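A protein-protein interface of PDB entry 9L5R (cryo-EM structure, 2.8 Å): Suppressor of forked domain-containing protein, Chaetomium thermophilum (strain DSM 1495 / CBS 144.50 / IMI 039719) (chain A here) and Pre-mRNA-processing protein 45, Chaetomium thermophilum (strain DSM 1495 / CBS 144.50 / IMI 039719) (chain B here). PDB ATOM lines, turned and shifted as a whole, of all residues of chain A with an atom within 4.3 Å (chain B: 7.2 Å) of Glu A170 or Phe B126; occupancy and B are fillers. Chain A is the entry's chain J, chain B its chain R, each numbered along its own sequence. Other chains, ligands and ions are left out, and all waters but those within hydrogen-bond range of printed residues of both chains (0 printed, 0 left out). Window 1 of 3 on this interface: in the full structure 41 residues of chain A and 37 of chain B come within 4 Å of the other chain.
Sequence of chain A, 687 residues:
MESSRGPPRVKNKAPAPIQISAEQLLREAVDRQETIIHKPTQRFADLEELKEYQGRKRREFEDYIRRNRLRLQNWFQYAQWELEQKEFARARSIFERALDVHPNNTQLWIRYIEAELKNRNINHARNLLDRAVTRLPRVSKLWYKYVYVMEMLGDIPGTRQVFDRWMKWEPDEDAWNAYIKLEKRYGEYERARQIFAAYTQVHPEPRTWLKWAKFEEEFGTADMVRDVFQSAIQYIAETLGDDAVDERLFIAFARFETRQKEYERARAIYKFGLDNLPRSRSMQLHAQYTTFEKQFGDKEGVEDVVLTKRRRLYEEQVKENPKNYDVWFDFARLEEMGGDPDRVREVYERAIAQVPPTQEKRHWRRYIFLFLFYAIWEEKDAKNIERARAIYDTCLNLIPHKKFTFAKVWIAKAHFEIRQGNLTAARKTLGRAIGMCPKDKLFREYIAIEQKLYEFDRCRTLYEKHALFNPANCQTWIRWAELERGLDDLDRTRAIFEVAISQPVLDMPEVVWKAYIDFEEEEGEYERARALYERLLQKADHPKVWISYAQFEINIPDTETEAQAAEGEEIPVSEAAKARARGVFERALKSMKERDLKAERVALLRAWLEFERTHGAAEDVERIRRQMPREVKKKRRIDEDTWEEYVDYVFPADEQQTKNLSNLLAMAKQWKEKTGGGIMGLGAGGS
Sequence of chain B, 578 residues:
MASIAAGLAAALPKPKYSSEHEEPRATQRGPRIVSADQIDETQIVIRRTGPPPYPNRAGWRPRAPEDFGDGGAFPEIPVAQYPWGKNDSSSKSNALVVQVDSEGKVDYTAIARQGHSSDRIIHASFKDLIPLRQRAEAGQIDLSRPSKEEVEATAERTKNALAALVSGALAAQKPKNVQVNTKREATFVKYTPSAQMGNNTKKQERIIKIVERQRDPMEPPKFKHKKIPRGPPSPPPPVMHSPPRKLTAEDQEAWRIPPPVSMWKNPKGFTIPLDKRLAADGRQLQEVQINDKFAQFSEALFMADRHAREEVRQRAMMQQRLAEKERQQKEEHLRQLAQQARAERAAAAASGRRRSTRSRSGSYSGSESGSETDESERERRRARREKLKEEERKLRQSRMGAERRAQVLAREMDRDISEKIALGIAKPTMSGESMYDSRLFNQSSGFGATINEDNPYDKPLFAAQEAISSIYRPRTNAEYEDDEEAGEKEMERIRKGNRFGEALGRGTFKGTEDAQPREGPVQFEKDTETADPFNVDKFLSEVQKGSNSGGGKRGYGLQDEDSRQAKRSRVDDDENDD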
ATOM      1  N   ARG A 138      -0.475  -2.327 -27.969  1.00  0.00           N
ATOM      2  CA  ARG A 138      -1.847  -2.568 -28.460  1.00  0.00           C
ATOM      3  C   ARG A 138      -1.886  -2.327 -29.957  1.00  0.00           C
ATOM      4  O   ARG A 138      -2.978  -2.232 -30.486  1.00  0.00           O
ATOM      5  CB  ARG A 138      -2.843  -1.746 -27.651  1.00  0.00           C
ATOM      6  CG  ARG A 138      -3.040  -2.284 -26.248  1.00  0.00           C
ATOM      7  CD  ARG A 138      -4.318  -3.064 -26.351  1.00  0.00           C
ATOM      8  NE  ARG A 138      -4.432  -4.151 -25.403  1.00  0.00           N
ATOM      9  CZ  ARG A 138      -4.858  -4.020 -24.160  1.00  0.00           C
ATOM     10  NH1 ARG A 138      -5.189  -2.834 -23.686  1.00  0.00           N
ATOM     11  NH2 ARG A 138      -4.956  -5.082 -23.393  1.00  0.00           N
ATOM     12  N   TRP A 166       2.468 -11.536 -26.210  1.00  0.00           N
ATOM     13  CA  TRP A 166       1.262 -10.908 -26.740  1.00  0.00           C
ATOM     14  C   TRP A 166       0.022 -11.323 -25.950  1.00  0.00           C
ATOM     15  O   TRP A 166      -0.814 -10.481 -25.579  1.00  0.00           O
ATOM     16  CB  TRP A 166       1.129 -11.276 -28.215  1.00  0.00           C
ATOM     17  CG  TRP A 166       0.248 -10.418 -29.033  1.00  0.00           C
ATOM     18  CD1 TRP A 166      -0.431  -9.328 -28.632  1.00  0.00           C
ATOM     19  CD2 TRP A 166      -0.064 -10.602 -30.409  1.00  0.00           C
ATOM     20  NE1 TRP A 166      -1.134  -8.799 -29.663  1.00  0.00           N
ATOM     21  CE2 TRP A 166      -0.941  -9.572 -30.772  1.00  0.00           C
ATOM     22  CE3 TRP A 166       0.329 -11.526 -31.380  1.00  0.00           C
ATOM     23  CZ2 TRP A 166      -1.425  -9.431 -32.066  1.00  0.00           C
ATOM     24  CZ3 TRP A 166      -0.168 -11.397 -32.650  1.00  0.00           C
ATOM     25  CH2 TRP A 166      -1.030 -10.356 -32.984  1.00  0.00           C
ATOM     26  N   MET A 167      -0.081 -12.612 -25.627  1.00  0.00           N
ATOM     27  CA  MET A 167      -1.259 -13.093 -24.924  1.00  0.00           C
ATOM     28  C   MET A 167      -1.313 -12.533 -23.520  1.00  0.00           C
ATOM     29  O   MET A 167      -2.403 -12.340 -22.978  1.00  0.00           O
ATOM     30  CB  MET A 167      -1.280 -14.615 -24.839  1.00  0.00           C
ATOM     31  CG  MET A 167      -1.379 -15.348 -26.145  1.00  0.00           C
ATOM     32  SD  MET A 167      -2.781 -15.101 -27.212  1.00  0.00           S
ATOM     33  CE  MET A 167      -2.039 -14.044 -28.417  1.00  0.00           C
ATOM     34  N   LYS A 168      -0.147 -12.305 -22.909  1.00  0.00           N
ATOM     35  CA  LYS A 168      -0.096 -11.562 -21.656  1.00  0.00           C
ATOM     36  C   LYS A 168      -0.718 -10.188 -21.823  1.00  0.00           C
ATOM     37  O   LYS A 168      -1.443  -9.714 -20.948  1.00  0.00           O
ATOM     38  CB  LYS A 168       1.345 -11.423 -21.175  1.00  0.00           C
ATOM     39  CG  LYS A 168       1.826 -12.528 -20.295  1.00  0.00           C
ATOM     40  CD  LYS A 168       3.197 -12.224 -19.759  1.00  0.00           C
ATOM     41  CE  LYS A 168       4.277 -12.563 -20.772  1.00  0.00           C
ATOM     42  NZ  LYS A 168       4.443 -14.026 -21.008  1.00  0.00           N
ATOM     43  N   TRP A 169      -0.481  -9.550 -22.964  1.00  0.00           N
ATOM     44  CA  TRP A 169      -1.160  -8.276 -23.182  1.00  0.00           C
ATOM     45  C   TRP A 169      -2.645  -8.412 -23.483  1.00  0.00           C
ATOM     46  O   TRP A 169      -3.319  -7.389 -23.602  1.00  0.00           O
ATOM     47  CB  TRP A 169      -0.473  -7.486 -24.281  1.00  0.00           C
ATOM     48  CG  TRP A 169       0.571  -6.700 -23.699  1.00  0.00           C
ATOM     49  CD1 TRP A 169       1.878  -7.010 -23.627  1.00  0.00           C
ATOM     50  CD2 TRP A 169       0.400  -5.485 -22.983  1.00  0.00           C
ATOM     51  NE1 TRP A 169       2.554  -6.036 -22.953  1.00  0.00           N
ATOM     52  CE2 TRP A 169       1.664  -5.079 -22.549  1.00  0.00           C
ATOM     53  CE3 TRP A 169      -0.702  -4.670 -22.708  1.00  0.00           C
ATOM     54  CZ2 TRP A 169       1.860  -3.913 -21.839  1.00  0.00           C
ATOM     55  CZ3 TRP A 169      -0.505  -3.518 -22.008  1.00  0.00           C
ATOM     56  CH2 TRP A 169       0.763  -3.144 -21.587  1.00  0.00           C
ATOM     57  N   GLU A 170      -3.151  -9.629 -23.622  1.00  0.00           N
ATOM     58  CA  GLU A 170      -4.574  -9.965 -23.801  1.00  0.00           C
ATOM     59  C   GLU A 170      -5.153  -9.364 -25.066  1.00  0.00           C
ATOM     60  O   GLU A 170      -6.093  -8.568 -25.001  1.00  0.00           O
ATOM     61  CB  GLU A 170      -5.461  -9.510 -22.643  1.00  0.00           C
ATOM     62  CG  GLU A 170      -5.408 -10.334 -21.416  1.00  0.00           C
ATOM     63  CD  GLU A 170      -6.642 -10.144 -20.570  1.00  0.00           C
ATOM     64  OE1 GLU A 170      -7.552  -9.423 -21.008  1.00  0.00           O
ATOM     65  OE2 GLU A 170      -6.698 -10.698 -19.457  1.00  0.00           O
ATOM     66  N   PRO A 171      -4.663  -9.748 -26.208  1.00  0.00           N
ATOM     67  CA  PRO A 171      -5.078  -9.102 -27.447  1.00  0.00           C
ATOM     68  C   PRO A 171      -6.458  -9.523 -27.894  1.00  0.00           C
ATOM     69  O   PRO A 171      -7.230 -10.118 -27.143  1.00  0.00           O
ATOM     70  CB  PRO A 171      -4.012  -9.556 -28.428  1.00  0.00           C
ATOM     71  CG  PRO A 171      -3.622 -10.855 -27.919  1.00  0.00           C
ATOM     72  CD  PRO A 171      -3.822 -10.917 -26.476  1.00  0.00           C
ATOM     73  N   ASP A 172      -6.791  -9.180 -29.121  1.00  0.00           N
ATOM     74  CA  ASP A 172      -8.091  -9.540 -29.624  1.00  0.00           C
ATOM     75  C   ASP A 172      -8.115 -10.968 -30.170  1.00  0.00           C
ATOM     76  O   ASP A 172      -7.112 -11.714 -30.214  1.00  0.00           O
ATOM     77  CB  ASP A 172      -8.539  -8.528 -30.670  1.00  0.00           C
ATOM     78  CG  ASP A 172      -8.497  -7.111 -30.151  1.00  0.00           C
ATOM     79  OD1 ASP A 172      -8.436  -6.928 -28.923  1.00  0.00           O
ATOM     80  OD2 ASP A 172      -8.548  -6.172 -30.962  1.00  0.00           O
ATOM     81  N   VAL A 202     -10.460 -15.150 -21.743  1.00  0.00           N
ATOM     82  CA  VAL A 202     -10.350 -13.732 -22.091  1.00  0.00           C
ATOM     83  C   VAL A 202     -11.544 -13.254 -22.923  1.00  0.00           C
ATOM     84  O   VAL A 202     -12.045 -12.146 -22.724  1.00  0.00           O
ATOM     85  CB  VAL A 202      -9.010 -13.475 -22.800  1.00  0.00           C
ATOM     86  CG1 VAL A 202      -8.891 -12.032 -23.241  1.00  0.00           C
ATOM     87  CG2 VAL A 202      -7.887 -13.806 -21.875  1.00  0.00           C
ATOM     88  N   ALA B 124       4.149  -0.516 -17.689  1.00  0.00           N
ATOM     89  CA  ALA B 124       4.586  -1.314 -18.824  1.00  0.00           C
ATOM     90  C   ALA B 124       3.854  -2.641 -18.915  1.00  0.00           C
ATOM     91  O   ALA B 124       4.315  -3.535 -19.620  1.00  0.00           O
ATOM     92  CB  ALA B 124       6.092  -1.557 -18.762  1.00  0.00           C
ATOM     93  N   SER B 125       2.873  -2.901 -18.081  1.00  0.00           N
ATOM     94  CA  SER B 125       2.282  -4.253 -18.095  1.00  0.00           C
ATOM     95  C   SER B 125       0.773  -4.161 -18.122  1.00  0.00           C
ATOM     96  O   SER B 125       0.245  -3.110 -17.807  1.00  0.00           O
ATOM     97  CB  SER B 125       2.726  -4.976 -16.906  1.00  0.00           C
ATOM     98  OG  SER B 125       4.066  -5.404 -17.058  1.00  0.00           O
ATOM     99  N   PHE B 126       0.120  -5.255 -18.465  1.00  0.00           N
ATOM    100  CA  PHE B 126      -1.353  -5.264 -18.507  1.00  0.00           C
ATOM    101  C   PHE B 126      -1.866  -5.000 -17.106  1.00  0.00           C
ATOM    102  O   PHE B 126      -2.968  -4.498 -16.964  1.00  0.00           O
ATOM    103  CB  PHE B 126      -1.875  -6.591 -19.039  1.00  0.00           C
ATOM    104  CG  PHE B 126      -3.367  -6.656 -19.193  1.00  0.00           C
ATOM    105  CD1 PHE B 126      -4.009  -5.907 -20.158  1.00  0.00           C
ATOM    106  CD2 PHE B 126      -4.127  -7.449 -18.357  1.00  0.00           C
ATOM    107  CE1 PHE B 126      -5.384  -5.956 -20.289  1.00  0.00           C
ATOM    108  CE2 PHE B 126      -5.502  -7.492 -18.487  1.00  0.00           C
ATOM    109  CZ  PHE B 126      -6.127  -6.747 -19.453  1.00  0.00           C
ATOM    110  N   LYS B 127      -1.067  -5.301 -16.102  1.00  0.00           N
ATOM    111  CA  LYS B 127      -1.540  -5.159 -14.718  1.00  0.00           C
ATOM    112  C   LYS B 127      -1.794  -3.693 -14.408  1.00  0.00           C
ATOM    113  O   LYS B 127      -2.607  -3.437 -13.543  1.00  0.00           O
ATOM    114  CB  LYS B 127      -0.507  -5.782 -13.791  1.00  0.00           C
ATOM    115  CG  LYS B 127       0.775  -4.995 -13.589  1.00  0.00           C
ATOM    116  CD  LYS B 127       1.646  -5.559 -12.496  1.00  0.00           C
ATOM    117  CE  LYS B 127       3.109  -5.598 -12.879  1.00  0.00           C
ATOM    118  NZ  LYS B 127       3.624  -4.250 -13.213  1.00  0.00           N
ATOM    119  N   ASP B 128      -1.169  -2.775 -15.124  1.00  0.00           N
ATOM    120  CA  ASP B 128      -1.303  -1.334 -14.844  1.00  0.00           C
ATOM    121  C   ASP B 128      -2.561  -0.814 -15.515  1.00  0.00           C
ATOM    122  O   ASP B 128      -2.872   0.340 -15.302  1.00  0.00           O
ATOM    123  CB  ASP B 128      -0.033  -0.628 -15.281  1.00  0.00           C
ATOM    124  CG  ASP B 128       1.215  -1.154 -14.607  1.00  0.00           C
ATOM    125  OD1 ASP B 128       1.218  -1.232 -13.373  1.00  0.00           O
ATOM    126  OD2 ASP B 128       2.169  -1.475 -15.325  1.00  0.00           O
ATOM    127  N   LEU B 129      -3.278  -1.671 -16.227  1.00  0.00           N
ATOM    128  CA  LEU B 129      -4.508  -1.280 -16.948  1.00  0.00           C
ATOM    129  C   LEU B 129      -5.715  -1.879 -16.244  1.00  0.00           C
ATOM    130  O   LEU B 129      -6.816  -1.536 -16.639  1.00  0.00           O
ATOM    131  CB  LEU B 129      -4.419  -1.810 -18.377  1.00  0.00           C
ATOM    132  CG  LEU B 129      -3.673  -0.950 -19.387  1.00  0.00           C
ATOM    133  CD1 LEU B 129      -3.476  -1.729 -20.669  1.00  0.00           C
ATOM    134  CD2 LEU B 129      -4.452   0.313 -19.678  1.00  0.00           C
ATOM    135  N   ILE B 130      -5.512  -2.731 -15.245  1.00  0.00           N
ATOM    136  CA  ILE B 130      -6.632  -3.335 -14.469  1.00  0.00           C
ATOM    137  C   ILE B 130      -6.960  -2.412 -13.310  1.00  0.00           C
ATOM    138  O   ILE B 130      -6.032  -2.040 -12.611  1.00  0.00           O
ATOM    139  CB  ILE B 130      -6.237  -4.726 -13.955  1.00  0.00           C
ATOM    140  CG1 ILE B 130      -5.782  -5.642 -15.088  1.00  0.00           C
ATOM    141  CG2 ILE B 130      -7.355  -5.358 -13.146  1.00  0.00           C
ATOM    142  CD1 ILE B 130      -4.996  -6.829 -14.603  1.00  0.00           C
ATOM    143  N   PRO B 131      -8.223  -2.026 -13.068  1.00  0.00           N
ATOM    144  CA  PRO B 131      -8.537  -1.203 -11.916  1.00  0.00           C
ATOM    145  C   PRO B 131      -7.938  -1.719 -10.609  1.00  0.00           C
ATOM    146  O   PRO B 131      -8.093  -2.856 -10.357  1.00  0.00           O
ATOM    147  CB  PRO B 131     -10.037  -1.344 -11.906  1.00  0.00           C
ATOM    148  CG  PRO B 131     -10.401  -1.373 -13.346  1.00  0.00           C
ATOM    149  CD  PRO B 131      -9.364  -2.302 -13.921  1.00  0.00           C
ATOM    150  N   ARG B 135      -7.249  -5.703  -8.593  1.00  0.00           N
ATOM    151  CA  ARG B 135      -5.919  -6.340  -8.670  1.00  0.00           C
ATOM    152  C   ARG B 135      -5.839  -7.303  -7.496  1.00  0.00           C
ATOM    153  O   ARG B 135      -6.032  -6.848  -6.360  1.00  0.00           O
ATOM    154  CB  ARG B 135      -4.820  -5.281  -8.733  1.00  0.00           C
ATOM    155  CG  ARG B 135      -4.724  -4.591 -10.084  1.00  0.00           C
ATOM    156  CD  ARG B 135      -3.531  -3.668 -10.154  1.00  0.00           C
ATOM    157  NE  ARG B 135      -3.881  -2.431 -10.828  1.00  0.00           N
ATOM    158  CZ  ARG B 135      -3.050  -1.423 -11.032  1.00  0.00           C
ATOM    159  NH1 ARG B 135      -1.801  -1.496 -10.614  1.00  0.00           N
ATOM    160  NH2 ARG B 135      -3.471  -0.344 -11.663  1.00  0.00           N
ATOM    161  N   MET B 240      -0.109   3.056 -23.246  1.00  0.00           N
ATOM    162  CA  MET B 240      -0.961   2.126 -22.509  1.00  0.00           C
ATOM    163  C   MET B 240      -2.425   2.317 -22.873  1.00  0.00           C
ATOM    164  O   MET B 240      -3.250   2.673 -22.051  1.00  0.00           O
ATOM    165  CB  MET B 240      -0.736   2.293 -21.013  1.00  0.00           C
ATOM    166  CG  MET B 240       0.716   2.149 -20.617  1.00  0.00           C
ATOM    167  SD  MET B 240       1.300   0.461 -20.703  1.00  0.00           S
ATOM    168  CE  MET B 240       0.148  -0.245 -19.569  1.00  0.00           C
ATOM    169  N   PRO B 243      -7.954  -1.592 -25.870  1.00  0.00           N
ATOM    170  CA  PRO B 243      -7.967  -2.205 -27.169  1.00  0.00           C
ATOM    171  C   PRO B 243      -8.563  -1.279 -28.230  1.00  0.00           C
ATOM    172  O   PRO B 243      -9.527  -0.632 -27.974  1.00  0.00           O
ATOM    173  CB  PRO B 243      -8.874  -3.390 -26.914  1.00  0.00           C
ATOM    174  CG  PRO B 243      -8.597  -3.759 -25.501  1.00  0.00           C
ATOM    175  CD  PRO B 243      -8.578  -2.408 -24.838  1.00  0.00           C
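Among the printed residues, 10 pairs touch across the chains. Among the printed residues, no Asp or Glu carboxylate lies within 4 Å of a Lys or Arg side-chain nitrogen of the other chain.
NH2 of Arg A138 touches CE1 of Phe B126 (3.3 Å). CD1 of Leu B129 touches NH1 of Arg A138, 3.6 Å away. Pro B243 touches Arg A138 (CD to NH1, 3.6 Å). Phe B126 touches Lys A168. Trp A169 touches Ala B124. C of Ser B125 touches CH2 of Trp A169, at 3.6 Å. O of Trp A169 touches CD1 of Phe B126 (3.8 Å). Leu B129 touches Trp A169 (CD1 to CZ3, 3.7 Å). Trp A169 touches Met B240. Phe B126 touches Glu A170.
Printed residues of chain B within 4 Å of Glu A170: Phe B126 (3.4 Å). Phe B126 touches just these residues of chain A: Arg A138, Lys A168, Trp A169 and Glu A170. Of the printed residues of chain A, Leu B129 touches Arg A138 and Trp A169. Of the printed residues of chain A, Met B240 touches Trp A169. Of the printed residues of chain B, Arg A138 touches Phe B126, Leu B129 and Pro B243. Printed residues of chain A within 4 Å of Pro B243: Arg A138 (3.6 Å). The nearest residue of chain B that does not touch Glu A170 is Pro B243 (5.4 Å).
The guanidinium group of Arg A138 sits at hydrogen-bond distance from the backbone carbonyl oxygen of Trp A169 (2.8 Å). OD2 of Asp B128 is in hydrogen-bond range of N of Ala B124 (3.2 Å). The backbone NH (N) of Ser B125 is in hydrogen-bond range of the side-chain carboxylate (OD2) of Asp B128, at 3.2 Å.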
